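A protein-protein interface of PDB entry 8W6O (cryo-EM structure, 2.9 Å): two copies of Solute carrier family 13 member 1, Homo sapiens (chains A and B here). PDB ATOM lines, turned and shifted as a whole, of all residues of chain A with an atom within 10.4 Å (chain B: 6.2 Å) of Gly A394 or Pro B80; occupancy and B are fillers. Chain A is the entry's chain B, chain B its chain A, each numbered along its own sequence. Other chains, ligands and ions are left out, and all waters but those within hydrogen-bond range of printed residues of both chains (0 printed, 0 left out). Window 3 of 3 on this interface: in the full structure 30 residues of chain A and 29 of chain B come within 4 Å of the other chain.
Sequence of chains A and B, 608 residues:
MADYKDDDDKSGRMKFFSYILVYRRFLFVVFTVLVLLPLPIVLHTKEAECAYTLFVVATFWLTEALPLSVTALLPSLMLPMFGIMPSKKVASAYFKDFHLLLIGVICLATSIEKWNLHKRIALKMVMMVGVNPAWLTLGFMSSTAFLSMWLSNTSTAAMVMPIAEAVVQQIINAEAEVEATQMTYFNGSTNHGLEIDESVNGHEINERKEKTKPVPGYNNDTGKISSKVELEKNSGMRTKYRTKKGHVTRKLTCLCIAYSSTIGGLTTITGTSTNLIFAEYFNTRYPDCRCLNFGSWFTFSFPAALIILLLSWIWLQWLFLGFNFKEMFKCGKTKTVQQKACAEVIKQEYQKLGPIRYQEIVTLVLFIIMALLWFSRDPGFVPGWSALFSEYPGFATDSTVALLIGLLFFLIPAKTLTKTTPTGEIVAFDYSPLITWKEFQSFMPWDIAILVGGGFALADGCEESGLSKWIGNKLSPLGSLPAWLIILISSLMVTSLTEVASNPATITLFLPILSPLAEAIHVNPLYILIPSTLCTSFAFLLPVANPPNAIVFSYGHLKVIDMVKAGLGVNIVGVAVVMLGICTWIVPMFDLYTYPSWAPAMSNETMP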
ATOM      1  N   PHE A  95      -2.159 -13.869 -18.258  1.00  0.00           N
ATOM      2  CA  PHE A  95      -3.165 -13.781 -17.206  1.00  0.00           C
ATOM      3  C   PHE A  95      -3.244 -12.385 -16.595  1.00  0.00           C
ATOM      4  O   PHE A  95      -2.296 -11.603 -16.671  1.00  0.00           O
ATOM      5  CB  PHE A  95      -2.903 -14.832 -16.122  1.00  0.00           C
ATOM      6  CG  PHE A  95      -1.447 -15.116 -15.884  1.00  0.00           C
ATOM      7  CD1 PHE A  95      -0.863 -16.267 -16.392  1.00  0.00           C
ATOM      8  CD2 PHE A  95      -0.660 -14.229 -15.177  1.00  0.00           C
ATOM      9  CE1 PHE A  95       0.476 -16.533 -16.181  1.00  0.00           C
ATOM     10  CE2 PHE A  95       0.679 -14.489 -14.965  1.00  0.00           C
ATOM     11  CZ  PHE A  95       1.248 -15.643 -15.469  1.00  0.00           C
ATOM     12  N   LYS A  96      -4.387 -12.096 -15.975  1.00  0.00           N
ATOM     13  CA  LYS A  96      -4.787 -10.744 -15.629  1.00  0.00           C
ATOM     14  C   LYS A  96      -4.395 -10.395 -14.195  1.00  0.00           C
ATOM     15  O   LYS A  96      -3.924 -11.236 -13.427  1.00  0.00           O
ATOM     16  CB  LYS A  96      -6.289 -10.580 -15.848  1.00  0.00           C
ATOM     17  CG  LYS A  96      -6.704 -10.850 -17.281  1.00  0.00           C
ATOM     18  CD  LYS A  96      -6.110  -9.811 -18.219  1.00  0.00           C
ATOM     19  CE  LYS A  96      -6.564 -10.031 -19.647  1.00  0.00           C
ATOM     20  NZ  LYS A  96      -5.944 -11.259 -20.213  1.00  0.00           N
ATOM     21  N   ASP A  97      -4.613  -9.125 -13.833  1.00  0.00           N
ATOM     22  CA  ASP A  97      -4.095  -8.576 -12.584  1.00  0.00           C
ATOM     23  C   ASP A  97      -4.801  -9.139 -11.358  1.00  0.00           C
ATOM     24  O   ASP A  97      -4.203  -9.194 -10.274  1.00  0.00           O
ATOM     25  CB  ASP A  97      -4.221  -7.055 -12.598  1.00  0.00           C
ATOM     26  CG  ASP A  97      -3.391  -6.412 -13.686  1.00  0.00           C
ATOM     27  OD1 ASP A  97      -2.668  -7.140 -14.393  1.00  0.00           O
ATOM     28  OD2 ASP A  97      -3.465  -5.175 -13.835  1.00  0.00           O
ATOM     29  N   LEU A 100      -3.069 -12.248 -10.209  1.00  0.00           N
ATOM     30  CA  LEU A 100      -1.828 -11.881  -9.532  1.00  0.00           C
ATOM     31  C   LEU A 100      -2.089 -11.422  -8.102  1.00  0.00           C
ATOM     32  O   LEU A 100      -1.376 -11.824  -7.172  1.00  0.00           O
ATOM     33  CB  LEU A 100      -1.119 -10.780 -10.320  1.00  0.00           C
ATOM     34  CG  LEU A 100      -0.091 -11.096 -11.410  1.00  0.00           C
ATOM     35  CD1 LEU A 100      -0.740 -11.698 -12.623  1.00  0.00           C
ATOM     36  CD2 LEU A 100       0.634  -9.823 -11.800  1.00  0.00           C
ATOM     37  N   ARG A 290     -11.403   1.028 -15.215  1.00  0.00           N
ATOM     38  CA  ARG A 290     -10.380   1.060 -14.172  1.00  0.00           C
ATOM     39  C   ARG A 290     -10.918   1.947 -13.055  1.00  0.00           C
ATOM     40  O   ARG A 290     -10.561   3.122 -12.945  1.00  0.00           O
ATOM     41  CB  ARG A 290      -9.042   1.577 -14.719  1.00  0.00           C
ATOM     42  CG  ARG A 290      -8.312   0.625 -15.655  1.00  0.00           C
ATOM     43  CD  ARG A 290      -8.646   0.916 -17.113  1.00  0.00           C
ATOM     44  NE  ARG A 290      -7.594   0.485 -18.030  1.00  0.00           N
ATOM     45  CZ  ARG A 290      -7.448  -0.759 -18.478  1.00  0.00           C
ATOM     46  NH1 ARG A 290      -8.288  -1.712 -18.094  1.00  0.00           N
ATOM     47  NH2 ARG A 290      -6.459  -1.048 -19.310  1.00  0.00           N
ATOM     48  N   ARG A 377      -1.818   4.129  -2.156  1.00  0.00           N
ATOM     49  CA  ARG A 377      -1.778   4.458  -3.576  1.00  0.00           C
ATOM     50  C   ARG A 377      -3.183   4.509  -4.172  1.00  0.00           C
ATOM     51  O   ARG A 377      -3.655   5.565  -4.596  1.00  0.00           O
ATOM     52  CB  ARG A 377      -0.922   3.447  -4.337  1.00  0.00           C
ATOM     53  CG  ARG A 377      -1.457   2.032  -4.307  1.00  0.00           C
ATOM     54  CD  ARG A 377      -0.986   1.243  -5.511  1.00  0.00           C
ATOM     55  NE  ARG A 377      -1.477   1.812  -6.761  1.00  0.00           N
ATOM     56  CZ  ARG A 377      -2.627   1.477  -7.336  1.00  0.00           C
ATOM     57  NH1 ARG A 377      -3.415   0.574  -6.776  1.00  0.00           N
ATOM     58  NH2 ARG A 377      -2.991   2.046  -8.475  1.00  0.00           N
ATOM     59  N   PHE A 389       1.567   5.460  -7.142  1.00  0.00           N
ATOM     60  CA  PHE A 389       2.544   6.317  -6.481  1.00  0.00           C
ATOM     61  C   PHE A 389       2.988   7.454  -7.404  1.00  0.00           C
ATOM     62  O   PHE A 389       2.196   7.967  -8.196  1.00  0.00           O
ATOM     63  CB  PHE A 389       3.759   5.500  -6.021  1.00  0.00           C
ATOM     64  CG  PHE A 389       3.410   4.318  -5.149  1.00  0.00           C
ATOM     65  CD1 PHE A 389       3.010   4.503  -3.832  1.00  0.00           C
ATOM     66  CD2 PHE A 389       3.494   3.021  -5.644  1.00  0.00           C
ATOM     67  CE1 PHE A 389       2.691   3.420  -3.029  1.00  0.00           C
ATOM     68  CE2 PHE A 389       3.175   1.935  -4.847  1.00  0.00           C
ATOM     69  CZ  PHE A 389       2.774   2.135  -3.540  1.00  0.00           C
ATOM     70  N   SER A 390       4.260   7.841  -7.294  1.00  0.00           N
ATOM     71  CA  SER A 390       4.780   8.973  -8.056  1.00  0.00           C
ATOM     72  C   SER A 390       5.267   8.549  -9.439  1.00  0.00           C
ATOM     73  O   SER A 390       4.909   9.168 -10.447  1.00  0.00           O
ATOM     74  CB  SER A 390       5.912   9.648  -7.280  1.00  0.00           C
ATOM     75  OG  SER A 390       5.433  10.226  -6.079  1.00  0.00           O
ATOM     76  N   GLU A 391       6.091   7.506  -9.502  1.00  0.00           N
ATOM     77  CA  GLU A 391       6.642   7.048 -10.769  1.00  0.00           C
ATOM     78  C   GLU A 391       5.572   6.355 -11.608  1.00  0.00           C
ATOM     79  O   GLU A 391       4.578   5.843 -11.088  1.00  0.00           O
ATOM     80  CB  GLU A 391       7.821   6.104 -10.524  1.00  0.00           C
ATOM     81  CG  GLU A 391       7.448   4.775  -9.884  1.00  0.00           C
ATOM     82  CD  GLU A 391       7.474   4.807  -8.367  1.00  0.00           C
ATOM     83  OE1 GLU A 391       7.522   5.909  -7.784  1.00  0.00           O
ATOM     84  OE2 GLU A 391       7.445   3.720  -7.754  1.00  0.00           O
ATOM     85  N   TYR A 392       5.774   6.362 -12.927  1.00  0.00           N
ATOM     86  CA  TYR A 392       4.716   5.870 -13.805  1.00  0.00           C
ATOM     87  C   TYR A 392       5.082   5.078 -15.071  1.00  0.00           C
ATOM     88  O   TYR A 392       4.494   5.378 -16.118  1.00  0.00           O
ATOM     89  CB  TYR A 392       3.904   7.096 -14.243  1.00  0.00           C
ATOM     90  CG  TYR A 392       4.777   8.307 -14.551  1.00  0.00           C
ATOM     91  CD1 TYR A 392       5.589   8.342 -15.685  1.00  0.00           C
ATOM     92  CD2 TYR A 392       4.801   9.407 -13.699  1.00  0.00           C
ATOM     93  CE1 TYR A 392       6.392   9.432 -15.963  1.00  0.00           C
ATOM     94  CE2 TYR A 392       5.604  10.508 -13.971  1.00  0.00           C
ATOM     95  CZ  TYR A 392       6.395  10.512 -15.106  1.00  0.00           C
ATOM     96  OH  TYR A 392       7.192  11.599 -15.385  1.00  0.00           O
ATOM     97  N   PRO A 393       6.014   4.072 -15.090  1.00  0.00           N
ATOM     98  CA  PRO A 393       6.076   3.260 -16.318  1.00  0.00           C
ATOM     99  C   PRO A 393       4.887   2.319 -16.489  1.00  0.00           C
ATOM    100  O   PRO A 393       4.062   2.524 -17.385  1.00  0.00           O
ATOM    101  CB  PRO A 393       7.393   2.484 -16.181  1.00  0.00           C
ATOM    102  CG  PRO A 393       7.760   2.548 -14.778  1.00  0.00           C
ATOM    103  CD  PRO A 393       7.143   3.763 -14.188  1.00  0.00           C
ATOM    104  N   GLY A 394       4.780   1.294 -15.643  1.00  0.00           N
ATOM    105  CA  GLY A 394       3.586   0.471 -15.592  1.00  0.00           C
ATOM    106  C   GLY A 394       3.333  -0.252 -14.283  1.00  0.00           C
ATOM    107  O   GLY A 394       2.383  -1.034 -14.189  1.00  0.00           O
ATOM    108  N   PHE A 395       4.161  -0.016 -13.265  1.00  0.00           N
ATOM    109  CA  PHE A 395       4.249  -0.931 -12.133  1.00  0.00           C
ATOM    110  C   PHE A 395       3.754  -0.337 -10.816  1.00  0.00           C
ATOM    111  O   PHE A 395       4.014  -0.906  -9.751  1.00  0.00           O
ATOM    112  CB  PHE A 395       5.684  -1.460 -11.999  1.00  0.00           C
ATOM    113  CG  PHE A 395       6.630  -0.536 -11.282  1.00  0.00           C
ATOM    114  CD1 PHE A 395       7.011   0.663 -11.847  1.00  0.00           C
ATOM    115  CD2 PHE A 395       7.171  -0.893 -10.054  1.00  0.00           C
ATOM    116  CE1 PHE A 395       7.891   1.502 -11.199  1.00  0.00           C
ATOM    117  CE2 PHE A 395       8.050  -0.054  -9.396  1.00  0.00           C
ATOM    118  CZ  PHE A 395       8.410   1.145  -9.970  1.00  0.00           C
ATOM    119  N   ALA A 396       2.982   0.747 -10.856  1.00  0.00           N
ATOM    120  CA  ALA A 396       2.441   1.338  -9.639  1.00  0.00           C
ATOM    121  C   ALA A 396       1.074   0.771  -9.274  1.00  0.00           C
ATOM    122  O   ALA A 396       0.254   1.475  -8.669  1.00  0.00           O
ATOM    123  CB  ALA A 396       2.375   2.858  -9.777  1.00  0.00           C
ATOM    124  N   THR A 397       0.807  -0.483  -9.628  1.00  0.00           N
ATOM    125  CA  THR A 397      -0.482  -1.116  -9.399  1.00  0.00           C
ATOM    126  C   THR A 397      -0.472  -1.943  -8.112  1.00  0.00           C
ATOM    127  O   THR A 397       0.507  -1.973  -7.365  1.00  0.00           O
ATOM    128  CB  THR A 397      -0.856  -1.978 -10.604  1.00  0.00           C
ATOM    129  OG1 THR A 397      -2.187  -2.480 -10.442  1.00  0.00           O
ATOM    130  CG2 THR A 397       0.115  -3.135 -10.756  1.00  0.00           C
ATOM    131  N   ASP A 398      -1.593  -2.615  -7.842  1.00  0.00           N
ATOM    132  CA  ASP A 398      -1.734  -3.457  -6.660  1.00  0.00           C
ATOM    133  C   ASP A 398      -1.196  -4.863  -6.872  1.00  0.00           C
ATOM    134  O   ASP A 398      -0.737  -5.495  -5.912  1.00  0.00           O
ATOM    135  CB  ASP A 398      -3.204  -3.549  -6.241  1.00  0.00           C
ATOM    136  CG  ASP A 398      -3.652  -2.361  -5.414  1.00  0.00           C
ATOM    137  OD1 ASP A 398      -2.858  -1.873  -4.586  1.00  0.00           O
ATOM    138  OD2 ASP A 398      -4.801  -1.912  -5.593  1.00  0.00           O
ATOM    139  N   SER A 399      -1.251  -5.369  -8.107  1.00  0.00           N
ATOM    140  CA  SER A 399      -0.720  -6.698  -8.390  1.00  0.00           C
ATOM    141  C   SER A 399       0.799  -6.725  -8.295  1.00  0.00           C
ATOM    142  O   SER A 399       1.376  -7.759  -7.943  1.00  0.00           O
ATOM    143  CB  SER A 399      -1.175  -7.159  -9.772  1.00  0.00           C
ATOM    144  OG  SER A 399      -0.571  -6.393 -10.797  1.00  0.00           O
ATOM    145  N   THR A 400       1.452  -5.595  -8.583  1.00  0.00           N
ATOM    146  CA  THR A 400       2.897  -5.488  -8.409  1.00  0.00           C
ATOM    147  C   THR A 400       3.278  -5.606  -6.940  1.00  0.00           C
ATOM    148  O   THR A 400       4.202  -6.348  -6.592  1.00  0.00           O
ATOM    149  CB  THR A 400       3.391  -4.165  -8.998  1.00  0.00           C
ATOM    150  OG1 THR A 400       3.313  -4.224 -10.427  1.00  0.00           O
ATOM    151  CG2 THR A 400       4.832  -3.879  -8.595  1.00  0.00           C
ATOM    152  N   VAL A 401       2.547  -4.907  -6.065  1.00  0.00           N
ATOM    153  CA  VAL A 401       2.775  -4.990  -4.622  1.00  0.00           C
ATOM    154  C   VAL A 401       2.494  -6.397  -4.115  1.00  0.00           C
ATOM    155  O   VAL A 401       3.273  -6.958  -3.328  1.00  0.00           O
ATOM    156  CB  VAL A 401       1.914  -3.939  -3.895  1.00  0.00           C
ATOM    157  CG1 VAL A 401       2.048  -4.068  -2.388  1.00  0.00           C
ATOM    158  CG2 VAL A 401       2.295  -2.541  -4.343  1.00  0.00           C
ATOM    159  N   LEU A 403       2.550  -9.381  -5.814  1.00  0.00           N
ATOM    160  CA  LEU A 403       3.597 -10.317  -6.219  1.00  0.00           C
ATOM    161  C   LEU A 403       4.931 -10.008  -5.550  1.00  0.00           C
ATOM    162  O   LEU A 403       5.597 -10.923  -5.054  1.00  0.00           O
ATOM    163  CB  LEU A 403       3.754 -10.312  -7.737  1.00  0.00           C
ATOM    164  CG  LEU A 403       3.274 -11.556  -8.480  1.00  0.00           C
ATOM    165  CD1 LEU A 403       1.816 -11.836  -8.206  1.00  0.00           C
ATOM    166  CD2 LEU A 403       3.519 -11.386  -9.965  1.00  0.00           C
ATOM    167  N   PRO B  75       8.322 -12.904 -14.931  1.00  0.00           N
ATOM    168  CA  PRO B  75       8.132 -11.936 -16.028  1.00  0.00           C
ATOM    169  C   PRO B  75       6.859 -11.114 -15.915  1.00  0.00           C
ATOM    170  O   PRO B  75       6.771 -10.056 -16.545  1.00  0.00           O
ATOM    171  CB  PRO B  75       8.118 -12.813 -17.289  1.00  0.00           C
ATOM    172  CG  PRO B  75       7.867 -14.169 -16.814  1.00  0.00           C
ATOM    173  CD  PRO B  75       8.547 -14.248 -15.503  1.00  0.00           C
ATOM    174  N   SER B  76       5.871 -11.557 -15.137  1.00  0.00           N
ATOM    175  CA  SER B  76       4.703 -10.723 -14.882  1.00  0.00           C
ATOM    176  C   SER B  76       5.012  -9.587 -13.917  1.00  0.00           C
ATOM    177  O   SER B  76       4.245  -8.622 -13.848  1.00  0.00           O
ATOM    178  CB  SER B  76       3.561 -11.577 -14.341  1.00  0.00           C
ATOM    179  OG  SER B  76       3.107 -12.473 -15.334  1.00  0.00           O
ATOM    180  N   LEU B  77       6.111  -9.686 -13.173  1.00  0.00           N
ATOM    181  CA  LEU B  77       6.546  -8.665 -12.231  1.00  0.00           C
ATOM    182  C   LEU B  77       7.641  -7.768 -12.792  1.00  0.00           C
ATOM    183  O   LEU B  77       7.618  -6.556 -12.564  1.00  0.00           O
ATOM    184  CB  LEU B  77       7.034  -9.330 -10.938  1.00  0.00           C
ATOM    185  CG  LEU B  77       7.643  -8.470  -9.830  1.00  0.00           C
ATOM    186  CD1 LEU B  77       6.569  -7.689  -9.097  1.00  0.00           C
ATOM    187  CD2 LEU B  77       8.429  -9.332  -8.863  1.00  0.00           C
ATOM    188  N   MET B  78       8.590  -8.334 -13.539  1.00  0.00           N
ATOM    189  CA  MET B  78       9.777  -7.601 -13.965  1.00  0.00           C
ATOM    190  C   MET B  78       9.623  -6.922 -15.318  1.00  0.00           C
ATOM    191  O   MET B  78      10.268  -5.899 -15.558  1.00  0.00           O
ATOM    192  CB  MET B  78      10.985  -8.537 -14.009  1.00  0.00           C
ATOM    193  CG  MET B  78      11.313  -9.187 -12.680  1.00  0.00           C
ATOM    194  SD  MET B  78      12.524 -10.511 -12.835  1.00  0.00           S
ATOM    195  CE  MET B  78      13.891  -9.620 -13.561  1.00  0.00           C
ATOM    196  N   LEU B  79       8.807  -7.461 -16.216  1.00  0.00           N
ATOM    197  CA  LEU B  79       8.604  -6.807 -17.508  1.00  0.00           C
ATOM    198  C   LEU B  79       7.772  -5.518 -17.457  1.00  0.00           C
ATOM    199  O   LEU B  79       8.098  -4.596 -18.215  1.00  0.00           O
ATOM    200  CB  LEU B  79       7.989  -7.782 -18.521  1.00  0.00           C
ATOM    201  CG  LEU B  79       8.893  -8.821 -19.188  1.00  0.00           C
ATOM    202  CD1 LEU B  79       8.051  -9.822 -19.956  1.00  0.00           C
ATOM    203  CD2 LEU B  79       9.906  -8.161 -20.103  1.00  0.00           C
ATOM    204  N   PRO B  80       6.700  -5.381 -16.647  1.00  0.00           N
ATOM    205  CA  PRO B  80       6.049  -4.060 -16.575  1.00  0.00           C
ATOM    206  C   PRO B  80       6.888  -2.971 -15.927  1.00  0.00           C
ATOM    207  O   PRO B  80       6.714  -1.798 -16.275  1.00  0.00           O
ATOM    208  CB  PRO B  80       4.779  -4.341 -15.762  1.00  0.00           C
ATOM    209  CG  PRO B  80       4.468  -5.721 -16.065  1.00  0.00           C
ATOM    210  CD  PRO B  80       5.793  -6.396 -16.061  1.00  0.00           C
ATOM    211  N   MET B  81       7.790  -3.305 -15.004  1.00  0.00           N
ATOM    212  CA  MET B  81       8.572  -2.267 -14.341  1.00  0.00           C
ATOM    213  C   MET B  81       9.677  -1.703 -15.225  1.00  0.00           C
ATOM    214  O   MET B  81      10.232  -0.650 -14.899  1.00  0.00           O
ATOM    215  CB  MET B  81       9.174  -2.794 -13.036  1.00  0.00           C
ATOM    216  CG  MET B  81      10.425  -3.636 -13.201  1.00  0.00           C
ATOM    217  SD  MET B  81      11.610  -3.428 -11.861  1.00  0.00           S
ATOM    218  CE  MET B  81      12.345  -1.854 -12.297  1.00  0.00           C
ATOM    219  N   PHE B  82      10.006  -2.372 -16.328  1.00  0.00           N
ATOM    220  CA  PHE B  82      10.991  -1.878 -17.278  1.00  0.00           C
ATOM    221  C   PHE B  82      10.371  -1.048 -18.390  1.00  0.00           C
ATOM    222  O   PHE B  82      11.096  -0.317 -19.075  1.00  0.00           O
ATOM    223  CB  PHE B  82      11.762  -3.047 -17.899  1.00  0.00           C
ATOM    224  CG  PHE B  82      12.744  -3.690 -16.969  1.00  0.00           C
ATOM    225  CD1 PHE B  82      13.456  -2.929 -16.061  1.00  0.00           C
ATOM    226  CD2 PHE B  82      12.963  -5.054 -17.010  1.00  0.00           C
ATOM    227  CE1 PHE B  82      14.355  -3.520 -15.200  1.00  0.00           C
ATOM    228  CE2 PHE B  82      13.866  -5.650 -16.153  1.00  0.00           C
ATOM    229  CZ  PHE B  82      14.565  -4.881 -15.251  1.00  0.00           C
ATOM    230  N   GLY B  83       9.062  -1.139 -18.583  1.00  0.00           N
ATOM    231  CA  GLY B  83       8.395  -0.475 -19.678  1.00  0.00           C
ATOM    232  C   GLY B  83       7.964  -1.380 -20.808  1.00  0.00           C
ATOM    233  O   GLY B  83       7.753  -0.888 -21.921  1.00  0.00           O
ATOM    234  N   ILE B  84       7.823  -2.679 -20.560  1.00  0.00           N
ATOM    235  CA  ILE B  84       7.483  -3.656 -21.588  1.00  0.00           C
ATOM    236  C   ILE B  84       6.133  -4.254 -21.217  1.00  0.00           C
ATOM    237  O   ILE B  84       6.032  -5.036 -20.264  1.00  0.00           O
ATOM    238  CB  ILE B  84       8.559  -4.742 -21.724  1.00  0.00           C
ATOM    239  CG1 ILE B  84       9.910  -4.112 -22.083  1.00  0.00           C
ATOM    240  CG2 ILE B  84       8.157  -5.771 -22.767  1.00  0.00           C
ATOM    241  CD1 ILE B  84      11.100  -4.921 -21.642  1.00  0.00           C
ATOM    242  N   MET B  85       5.100  -3.890 -21.964  1.00  0.00           N
ATOM    243  CA  MET B  85       3.730  -4.292 -21.695  1.00  0.00           C
ATOM    244  C   MET B  85       3.253  -5.309 -22.724  1.00  0.00           C
ATOM    245  O   MET B  85       3.754  -5.343 -23.854  1.00  0.00           O
ATOM    246  CB  MET B  85       2.804  -3.066 -21.714  1.00  0.00           C
ATOM    247  CG  MET B  85       3.377  -1.830 -21.032  1.00  0.00           C
ATOM    248  SD  MET B  85       3.757  -2.088 -19.290  1.00  0.00           S
ATOM    249  CE  MET B  85       2.131  -2.465 -18.641  1.00  0.00           C
ATOM    250  N   PRO B  86       2.284  -6.172 -22.368  1.00  0.00           N
ATOM    251  CA  PRO B  86       1.714  -7.080 -23.370  1.00  0.00           C
ATOM    252  C   PRO B  86       0.822  -6.359 -24.377  1.00  0.00           C
ATOM    253  O   PRO B  86       0.644  -6.866 -25.485  1.00  0.00           O
ATOM    254  CB  PRO B  86       0.894  -8.065 -22.530  1.00  0.00           C
ATOM    255  CG  PRO B  86       0.608  -7.343 -21.266  1.00  0.00           C
ATOM    256  CD  PRO B  86       1.811  -6.494 -21.010  1.00  0.00           C
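O of Phe A395 lies close to OG1 of Thr A400 (3.5 Å).
Among the printed residues, merely in contact across the chains: Phe A95 with Ser B76, Gly A394 with Pro B80, Phe A395 with Met B81 and Thr A400 with Leu B77.
Gly A394 touches just one residue of chain B: Pro B80. Of chain A, only Gly A394 (3.7 Å) comes within 4 Å of Pro B80. No residue of chain A comes within 4 Å of Gly B83. Printed residues of chain B within 4 Å of Thr A400: Leu B77. Printed residues of chain B within 4 Å of Phe A95: Ser B76 (3.2 Å). Of the printed residues of chain A, Met B81 touches Phe A395. Printed residues of chain A within 4 Å of Ser B76: Phe A95 (3.2 Å). Asp A97 touches none of the printed residues of chain B. The nearest residue of chain B that does not touch Gly A394 is Met B85 (4.5 Å). The nearest printed residue of chain A that does not touch Pro B80 is Phe A395 (4.3 Å).
Printed residues of chain B that touch a printed residue of chain A: Ser B76, Leu B77, Pro B80 and Met B81. Printed residues of chain A that touch a printed residue of chain B: Phe A95, Gly A394, Phe A395 and Thr A400. Hydrophobic or aromatic side chains of chain A that line the printed part of chain B: Phe A95 and Phe A395. Among the printed residues, no Asp or Glu carboxylate lies within 4 Å of a Lys or Arg side-chain nitrogen of the other chain.
No position is printed for both chains.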
